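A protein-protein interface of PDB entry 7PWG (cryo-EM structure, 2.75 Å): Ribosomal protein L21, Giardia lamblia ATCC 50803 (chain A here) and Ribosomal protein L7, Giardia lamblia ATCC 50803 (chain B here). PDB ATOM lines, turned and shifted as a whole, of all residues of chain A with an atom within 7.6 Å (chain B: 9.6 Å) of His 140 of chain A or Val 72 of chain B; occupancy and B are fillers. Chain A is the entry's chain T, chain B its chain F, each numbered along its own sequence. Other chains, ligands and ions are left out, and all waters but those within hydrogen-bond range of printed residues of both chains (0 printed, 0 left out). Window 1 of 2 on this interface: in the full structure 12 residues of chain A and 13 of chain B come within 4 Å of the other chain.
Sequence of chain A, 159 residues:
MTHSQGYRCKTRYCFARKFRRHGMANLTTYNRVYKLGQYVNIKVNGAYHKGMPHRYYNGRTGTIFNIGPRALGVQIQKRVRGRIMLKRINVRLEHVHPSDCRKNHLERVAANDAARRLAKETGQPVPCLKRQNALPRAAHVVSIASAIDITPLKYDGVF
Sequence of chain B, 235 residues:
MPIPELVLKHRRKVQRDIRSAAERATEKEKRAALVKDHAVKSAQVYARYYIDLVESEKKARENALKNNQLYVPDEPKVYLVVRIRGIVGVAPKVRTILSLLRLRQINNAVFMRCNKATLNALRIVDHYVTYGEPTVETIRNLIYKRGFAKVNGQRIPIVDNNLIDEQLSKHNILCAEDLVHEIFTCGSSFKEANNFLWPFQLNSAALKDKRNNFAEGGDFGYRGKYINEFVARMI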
ATOM      1  N   ARG A 137      -3.137  19.831  13.415  1.00  0.00           N
ATOM      2  CA  ARG A 137      -2.901  21.255  13.631  1.00  0.00           C
ATOM      3  C   ARG A 137      -2.085  21.498  14.895  1.00  0.00           C
ATOM      4  O   ARG A 137      -2.121  20.714  15.842  1.00  0.00           O
ATOM      5  CB  ARG A 137      -4.220  22.018  13.740  1.00  0.00           C
ATOM      6  CG  ARG A 137      -5.345  21.469  12.894  1.00  0.00           C
ATOM      7  CD  ARG A 137      -6.707  22.001  13.336  1.00  0.00           C
ATOM      8  NE  ARG A 137      -7.799  21.389  12.574  1.00  0.00           N
ATOM      9  CZ  ARG A 137      -8.707  20.558  13.084  1.00  0.00           C
ATOM     10  NH1 ARG A 137      -8.678  20.242  14.371  1.00  0.00           N
ATOM     11  NH2 ARG A 137      -9.652  20.049  12.312  1.00  0.00           N
ATOM     12  N   ALA A 138      -1.369  22.618  14.910  1.00  0.00           N
ATOM     13  CA  ALA A 138      -0.547  23.030  16.037  1.00  0.00           C
ATOM     14  C   ALA A 138      -1.354  23.830  17.057  1.00  0.00           C
ATOM     15  O   ALA A 138      -2.513  24.189  16.836  1.00  0.00           O
ATOM     16  CB  ALA A 138       0.643  23.853  15.556  1.00  0.00           C
ATOM     17  N   ALA A 139      -0.707  24.117  18.187  1.00  0.00           N
ATOM     18  CA  ALA A 139      -1.319  24.869  19.272  1.00  0.00           C
ATOM     19  C   ALA A 139      -1.391  26.355  18.946  1.00  0.00           C
ATOM     20  O   ALA A 139      -0.478  26.915  18.333  1.00  0.00           O
ATOM     21  CB  ALA A 139      -0.536  24.665  20.562  1.00  0.00           C
ATOM     22  N   HIS A 140      -2.479  26.995  19.367  1.00  0.00           N
ATOM     23  CA  HIS A 140      -2.717  28.399  19.066  1.00  0.00           C
ATOM     24  C   HIS A 140      -3.755  28.942  20.035  1.00  0.00           C
ATOM     25  O   HIS A 140      -4.434  28.193  20.733  1.00  0.00           O
ATOM     26  CB  HIS A 140      -3.179  28.577  17.622  1.00  0.00           C
ATOM     27  CG  HIS A 140      -4.352  27.724  17.265  1.00  0.00           C
ATOM     28  ND1 HIS A 140      -5.642  28.062  17.598  1.00  0.00           N
ATOM     29  CD2 HIS A 140      -4.427  26.528  16.641  1.00  0.00           C
ATOM     30  CE1 HIS A 140      -6.465  27.124  17.174  1.00  0.00           C
ATOM     31  NE2 HIS A 140      -5.753  26.180  16.590  1.00  0.00           N
ATOM     32  N   VAL A 141      -3.875  30.266  20.065  1.00  0.00           N
ATOM     33  CA  VAL A 141      -4.864  30.937  20.897  1.00  0.00           C
ATOM     34  C   VAL A 141      -5.958  31.509  20.005  1.00  0.00           C
ATOM     35  O   VAL A 141      -5.723  31.867  18.847  1.00  0.00           O
ATOM     36  CB  VAL A 141      -4.236  32.039  21.773  1.00  0.00           C
ATOM     37  CG1 VAL A 141      -3.258  31.442  22.759  1.00  0.00           C
ATOM     38  CG2 VAL A 141      -3.555  33.077  20.918  1.00  0.00           C
ATOM     39  N   VAL A 142      -7.170  31.569  20.548  1.00  0.00           N
ATOM     40  CA  VAL A 142      -8.317  32.145  19.856  1.00  0.00           C
ATOM     41  C   VAL A 142      -9.118  32.959  20.862  1.00  0.00           C
ATOM     42  O   VAL A 142      -9.232  32.578  22.030  1.00  0.00           O
ATOM     43  CB  VAL A 142      -9.195  31.061  19.181  1.00  0.00           C
ATOM     44  CG1 VAL A 142      -9.582  29.993  20.171  1.00  0.00           C
ATOM     45  CG2 VAL A 142     -10.439  31.671  18.575  1.00  0.00           C
ATOM     46  N   GLU B  57       1.872  24.355  29.434  1.00  0.00           N
ATOM     47  CA  GLU B  57       0.459  24.482  29.096  1.00  0.00           C
ATOM     48  C   GLU B  57      -0.291  25.228  30.187  1.00  0.00           C
ATOM     49  O   GLU B  57      -1.070  26.141  29.901  1.00  0.00           O
ATOM     50  CB  GLU B  57      -0.145  23.100  28.873  1.00  0.00           C
ATOM     51  CG  GLU B  57      -1.365  23.069  27.963  1.00  0.00           C
ATOM     52  CD  GLU B  57      -2.684  22.886  28.711  1.00  0.00           C
ATOM     53  OE1 GLU B  57      -2.772  23.278  29.893  1.00  0.00           O
ATOM     54  OE2 GLU B  57      -3.635  22.351  28.105  1.00  0.00           O
ATOM     55  N   ALA B  60      -0.019  28.718  29.979  1.00  0.00           N
ATOM     56  CA  ALA B  60      -0.607  29.227  28.743  1.00  0.00           C
ATOM     57  C   ALA B  60      -2.127  29.248  28.795  1.00  0.00           C
ATOM     58  O   ALA B  60      -2.752  30.166  28.260  1.00  0.00           O
ATOM     59  CB  ALA B  60      -0.132  28.397  27.550  1.00  0.00           C
ATOM     60  N   ARG B  61      -2.731  28.241  29.424  1.00  0.00           N
ATOM     61  CA  ARG B  61      -4.152  28.301  29.735  1.00  0.00           C
ATOM     62  C   ARG B  61      -4.451  29.423  30.715  1.00  0.00           C
ATOM     63  O   ARG B  61      -5.549  29.980  30.705  1.00  0.00           O
ATOM     64  CB  ARG B  61      -4.616  26.958  30.305  1.00  0.00           C
ATOM     65  CG  ARG B  61      -4.911  25.889  29.246  1.00  0.00           C
ATOM     66  CD  ARG B  61      -5.583  24.651  29.829  1.00  0.00           C
ATOM     67  NE  ARG B  61      -6.401  24.947  31.001  1.00  0.00           N
ATOM     68  CZ  ARG B  61      -7.594  25.538  30.964  1.00  0.00           C
ATOM     69  NH1 ARG B  61      -8.119  25.910  29.808  1.00  0.00           N
ATOM     70  NH2 ARG B  61      -8.254  25.768  32.085  1.00  0.00           N
ATOM     71  N   ALA B  64      -4.524  32.649  29.045  1.00  0.00           N
ATOM     72  CA  ALA B  64      -5.784  32.702  28.321  1.00  0.00           C
ATOM     73  C   ALA B  64      -6.851  33.412  29.143  1.00  0.00           C
ATOM     74  O   ALA B  64      -7.611  34.227  28.614  1.00  0.00           O
ATOM     75  CB  ALA B  64      -6.219  31.285  27.956  1.00  0.00           C
ATOM     76  N   GLN B  69      -9.888  34.806  26.205  1.00  0.00           N
ATOM     77  CA  GLN B  69      -9.235  33.952  25.225  1.00  0.00           C
ATOM     78  C   GLN B  69      -9.151  32.521  25.734  1.00  0.00           C
ATOM     79  O   GLN B  69      -9.164  32.257  26.937  1.00  0.00           O
ATOM     80  CB  GLN B  69      -7.830  34.460  24.878  1.00  0.00           C
ATOM     81  CG  GLN B  69      -7.806  35.648  23.948  1.00  0.00           C
ATOM     82  CD  GLN B  69      -6.408  35.996  23.471  1.00  0.00           C
ATOM     83  OE1 GLN B  69      -5.414  35.680  24.124  1.00  0.00           O
ATOM     84  NE2 GLN B  69      -6.326  36.640  22.320  1.00  0.00           N
ATOM     85  N   LEU B  70      -9.065  31.597  24.785  1.00  0.00           N
ATOM     86  CA  LEU B  70      -8.850  30.185  25.048  1.00  0.00           C
ATOM     87  C   LEU B  70      -7.468  29.795  24.555  1.00  0.00           C
ATOM     88  O   LEU B  70      -6.887  30.466  23.705  1.00  0.00           O
ATOM     89  CB  LEU B  70      -9.904  29.317  24.350  1.00  0.00           C
ATOM     90  CG  LEU B  70     -11.270  29.228  25.013  1.00  0.00           C
ATOM     91  CD1 LEU B  70     -12.151  28.188  24.340  1.00  0.00           C
ATOM     92  CD2 LEU B  70     -11.131  28.955  26.497  1.00  0.00           C
ATOM     93  N   TYR B  71      -6.938  28.710  25.097  1.00  0.00           N
ATOM     94  CA  TYR B  71      -5.711  28.116  24.593  1.00  0.00           C
ATOM     95  C   TYR B  71      -6.047  26.757  24.004  1.00  0.00           C
ATOM     96  O   TYR B  71      -6.512  25.867  24.717  1.00  0.00           O
ATOM     97  CB  TYR B  71      -4.659  27.985  25.689  1.00  0.00           C
ATOM     98  CG  TYR B  71      -3.392  27.292  25.236  1.00  0.00           C
ATOM     99  CD1 TYR B  71      -2.472  27.949  24.433  1.00  0.00           C
ATOM    100  CD2 TYR B  71      -3.118  25.987  25.611  1.00  0.00           C
ATOM    101  CE1 TYR B  71      -1.316  27.329  24.017  1.00  0.00           C
ATOM    102  CE2 TYR B  71      -1.974  25.360  25.198  1.00  0.00           C
ATOM    103  CZ  TYR B  71      -1.071  26.034  24.407  1.00  0.00           C
ATOM    104  OH  TYR B  71       0.079  25.403  24.001  1.00  0.00           O
ATOM    105  N   VAL B  72      -5.802  26.601  22.710  1.00  0.00           N
ATOM    106  CA  VAL B  72      -6.104  25.377  21.982  1.00  0.00           C
ATOM    107  C   VAL B  72      -4.784  24.651  21.740  1.00  0.00           C
ATOM    108  O   VAL B  72      -3.962  25.117  20.944  1.00  0.00           O
ATOM    109  CB  VAL B  72      -6.841  25.679  20.669  1.00  0.00           C
ATOM    110  CG1 VAL B  72      -7.319  24.410  20.002  1.00  0.00           C
ATOM    111  CG2 VAL B  72      -8.010  26.579  20.941  1.00  0.00           C
ATOM    112  N   PRO B  73      -4.529  23.530  22.409  1.00  0.00           N
ATOM    113  CA  PRO B  73      -3.243  22.831  22.257  1.00  0.00           C
ATOM    114  C   PRO B  73      -3.100  21.993  20.992  1.00  0.00           C
ATOM    115  O   PRO B  73      -3.957  22.015  20.106  1.00  0.00           O
ATOM    116  CB  PRO B  73      -3.196  21.942  23.500  1.00  0.00           C
ATOM    117  CG  PRO B  73      -4.633  21.742  23.859  1.00  0.00           C
ATOM    118  CD  PRO B  73      -5.307  23.018  23.546  1.00  0.00           C
ATOM    119  N   ASP B  74      -1.996  21.255  20.895  1.00  0.00           N
ATOM    120  CA  ASP B  74      -1.748  20.426  19.729  1.00  0.00           C
ATOM    121  C   ASP B  74      -2.565  19.143  19.789  1.00  0.00           C
ATOM    122  O   ASP B  74      -2.834  18.592  20.860  1.00  0.00           O
ATOM    123  CB  ASP B  74      -0.264  20.085  19.597  1.00  0.00           C
ATOM    124  CG  ASP B  74       0.078  19.465  18.243  1.00  0.00           C
ATOM    125  OD1 ASP B  74       0.210  20.216  17.261  1.00  0.00           O
ATOM    126  OD2 ASP B  74       0.207  18.230  18.146  1.00  0.00           O
ATOM    127  N   GLU B  75      -2.965  18.681  18.616  1.00  0.00           N
ATOM    128  CA  GLU B  75      -3.695  17.439  18.479  1.00  0.00           C
ATOM    129  C   GLU B  75      -2.755  16.252  18.648  1.00  0.00           C
ATOM    130  O   GLU B  75      -1.540  16.396  18.643  1.00  0.00           O
ATOM    131  CB  GLU B  75      -4.400  17.433  17.132  1.00  0.00           C
ATOM    132  CG  GLU B  75      -5.455  18.491  17.069  1.00  0.00           C
ATOM    133  CD  GLU B  75      -6.028  18.642  15.709  1.00  0.00           C
ATOM    134  OE1 GLU B  75      -5.291  18.416  14.741  1.00  0.00           O
ATOM    135  OE2 GLU B  75      -7.215  18.992  15.602  1.00  0.00           O
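Among the printed residues, merely in contact across the chains: Ala 139 of chain A with Val 72 of chain B (3.1 Å), Ala 138 of chain A with Asp 74 of chain B (3.2 Å), Val 142 of chain A with Gln 69 of chain B (3.5 Å), Val 141 of chain A with Leu 70 of chain B (3.5 Å), Ala 139 of chain A with Tyr 71 of chain B (3.6 Å), Ala 139 of chain A with Pro 73 of chain B (3.7 Å), Ala 139 of chain A with Asp 74 of chain B (3.7 Å), Val 142 of chain A with Val 72 of chain B (3.8 Å), His 140 of chain A with Tyr 71 of chain B (3.9 Å) and Val 141 of chain A with Tyr 71 of chain B (3.95 Å).
N of His 140 of chain A is in hydrogen-bond range of O of Val 72 of chain B (2.9 Å). O of Val 142 of chain A lies within hydrogen-bond range of N of Leu 70 of chain B (2.9 Å). The side-chain carboxylate of Glu 75 of chain B is in salt-bridge range of the guanidinium group of Arg 137 of chain A (3.9 Å). O of Arg 137 of chain A sits close to OD1 of Asp 74 of chain B.
The backbone carbonyl oxygen (O) of Ala 64 of chain B is in hydrogen-bond range of the backbone NH (N) of Gln 69 of chain B, at 3.4 Å.
Printed residues of chain B that touch a printed residue of chain A: Gln 69, Leu 70, Tyr 71, Val 72, Pro 73, Asp 74 and Glu 75. Hydrophobic or aromatic side chains of chain B that line the printed part of chain A: Tyr 71 and Val 72. Along chain B the printed residues that touch a printed residue of chain A span positions 69 to 75. Among the printed residues, 14 pairs touch across the chains. Among the printed residues, Asp or Glu carboxylates within 4 Å of a Lys or Arg side-chain nitrogen of the other chain: Arg 137 of chain A with Glu 75 of chain B (2.3 Å).
Of the printed residues of chain B, Arg 137 of chain A touches Asp 74 (2.8 Å) and Glu 75 (2.3 Å). Of chain B, only Tyr 71 (3.6 Å), Val 72 (3.1 Å), Pro 73 (3.7 Å) and Asp 74 (3.7 Å) come within 4 Å of Ala 139 of chain A. His 140 of chain A touches just these residues of chain B: Tyr 71 and Val 72. Of the printed residues of chain B, Val 141 of chain A touches Leu 70 (3.5 Å) and Tyr 71 (3.95 Å). Printed residues of chain A within 4 Å of Gln 69 of chain B: Val 142. Printed residues of chain A within 4 Å of Leu 70 of chain B: Val 141 and Val 142. Of the printed residues of chain A, Asp 74 of chain B touches Arg 137, Ala 138 and Ala 139. Printed residues of chain A within 4 Å of Glu 75 of chain B: Arg 137. The nearest residue of chain B that does not touch His 140 of chain A is Leu 70 of chain B (4.5 Å).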
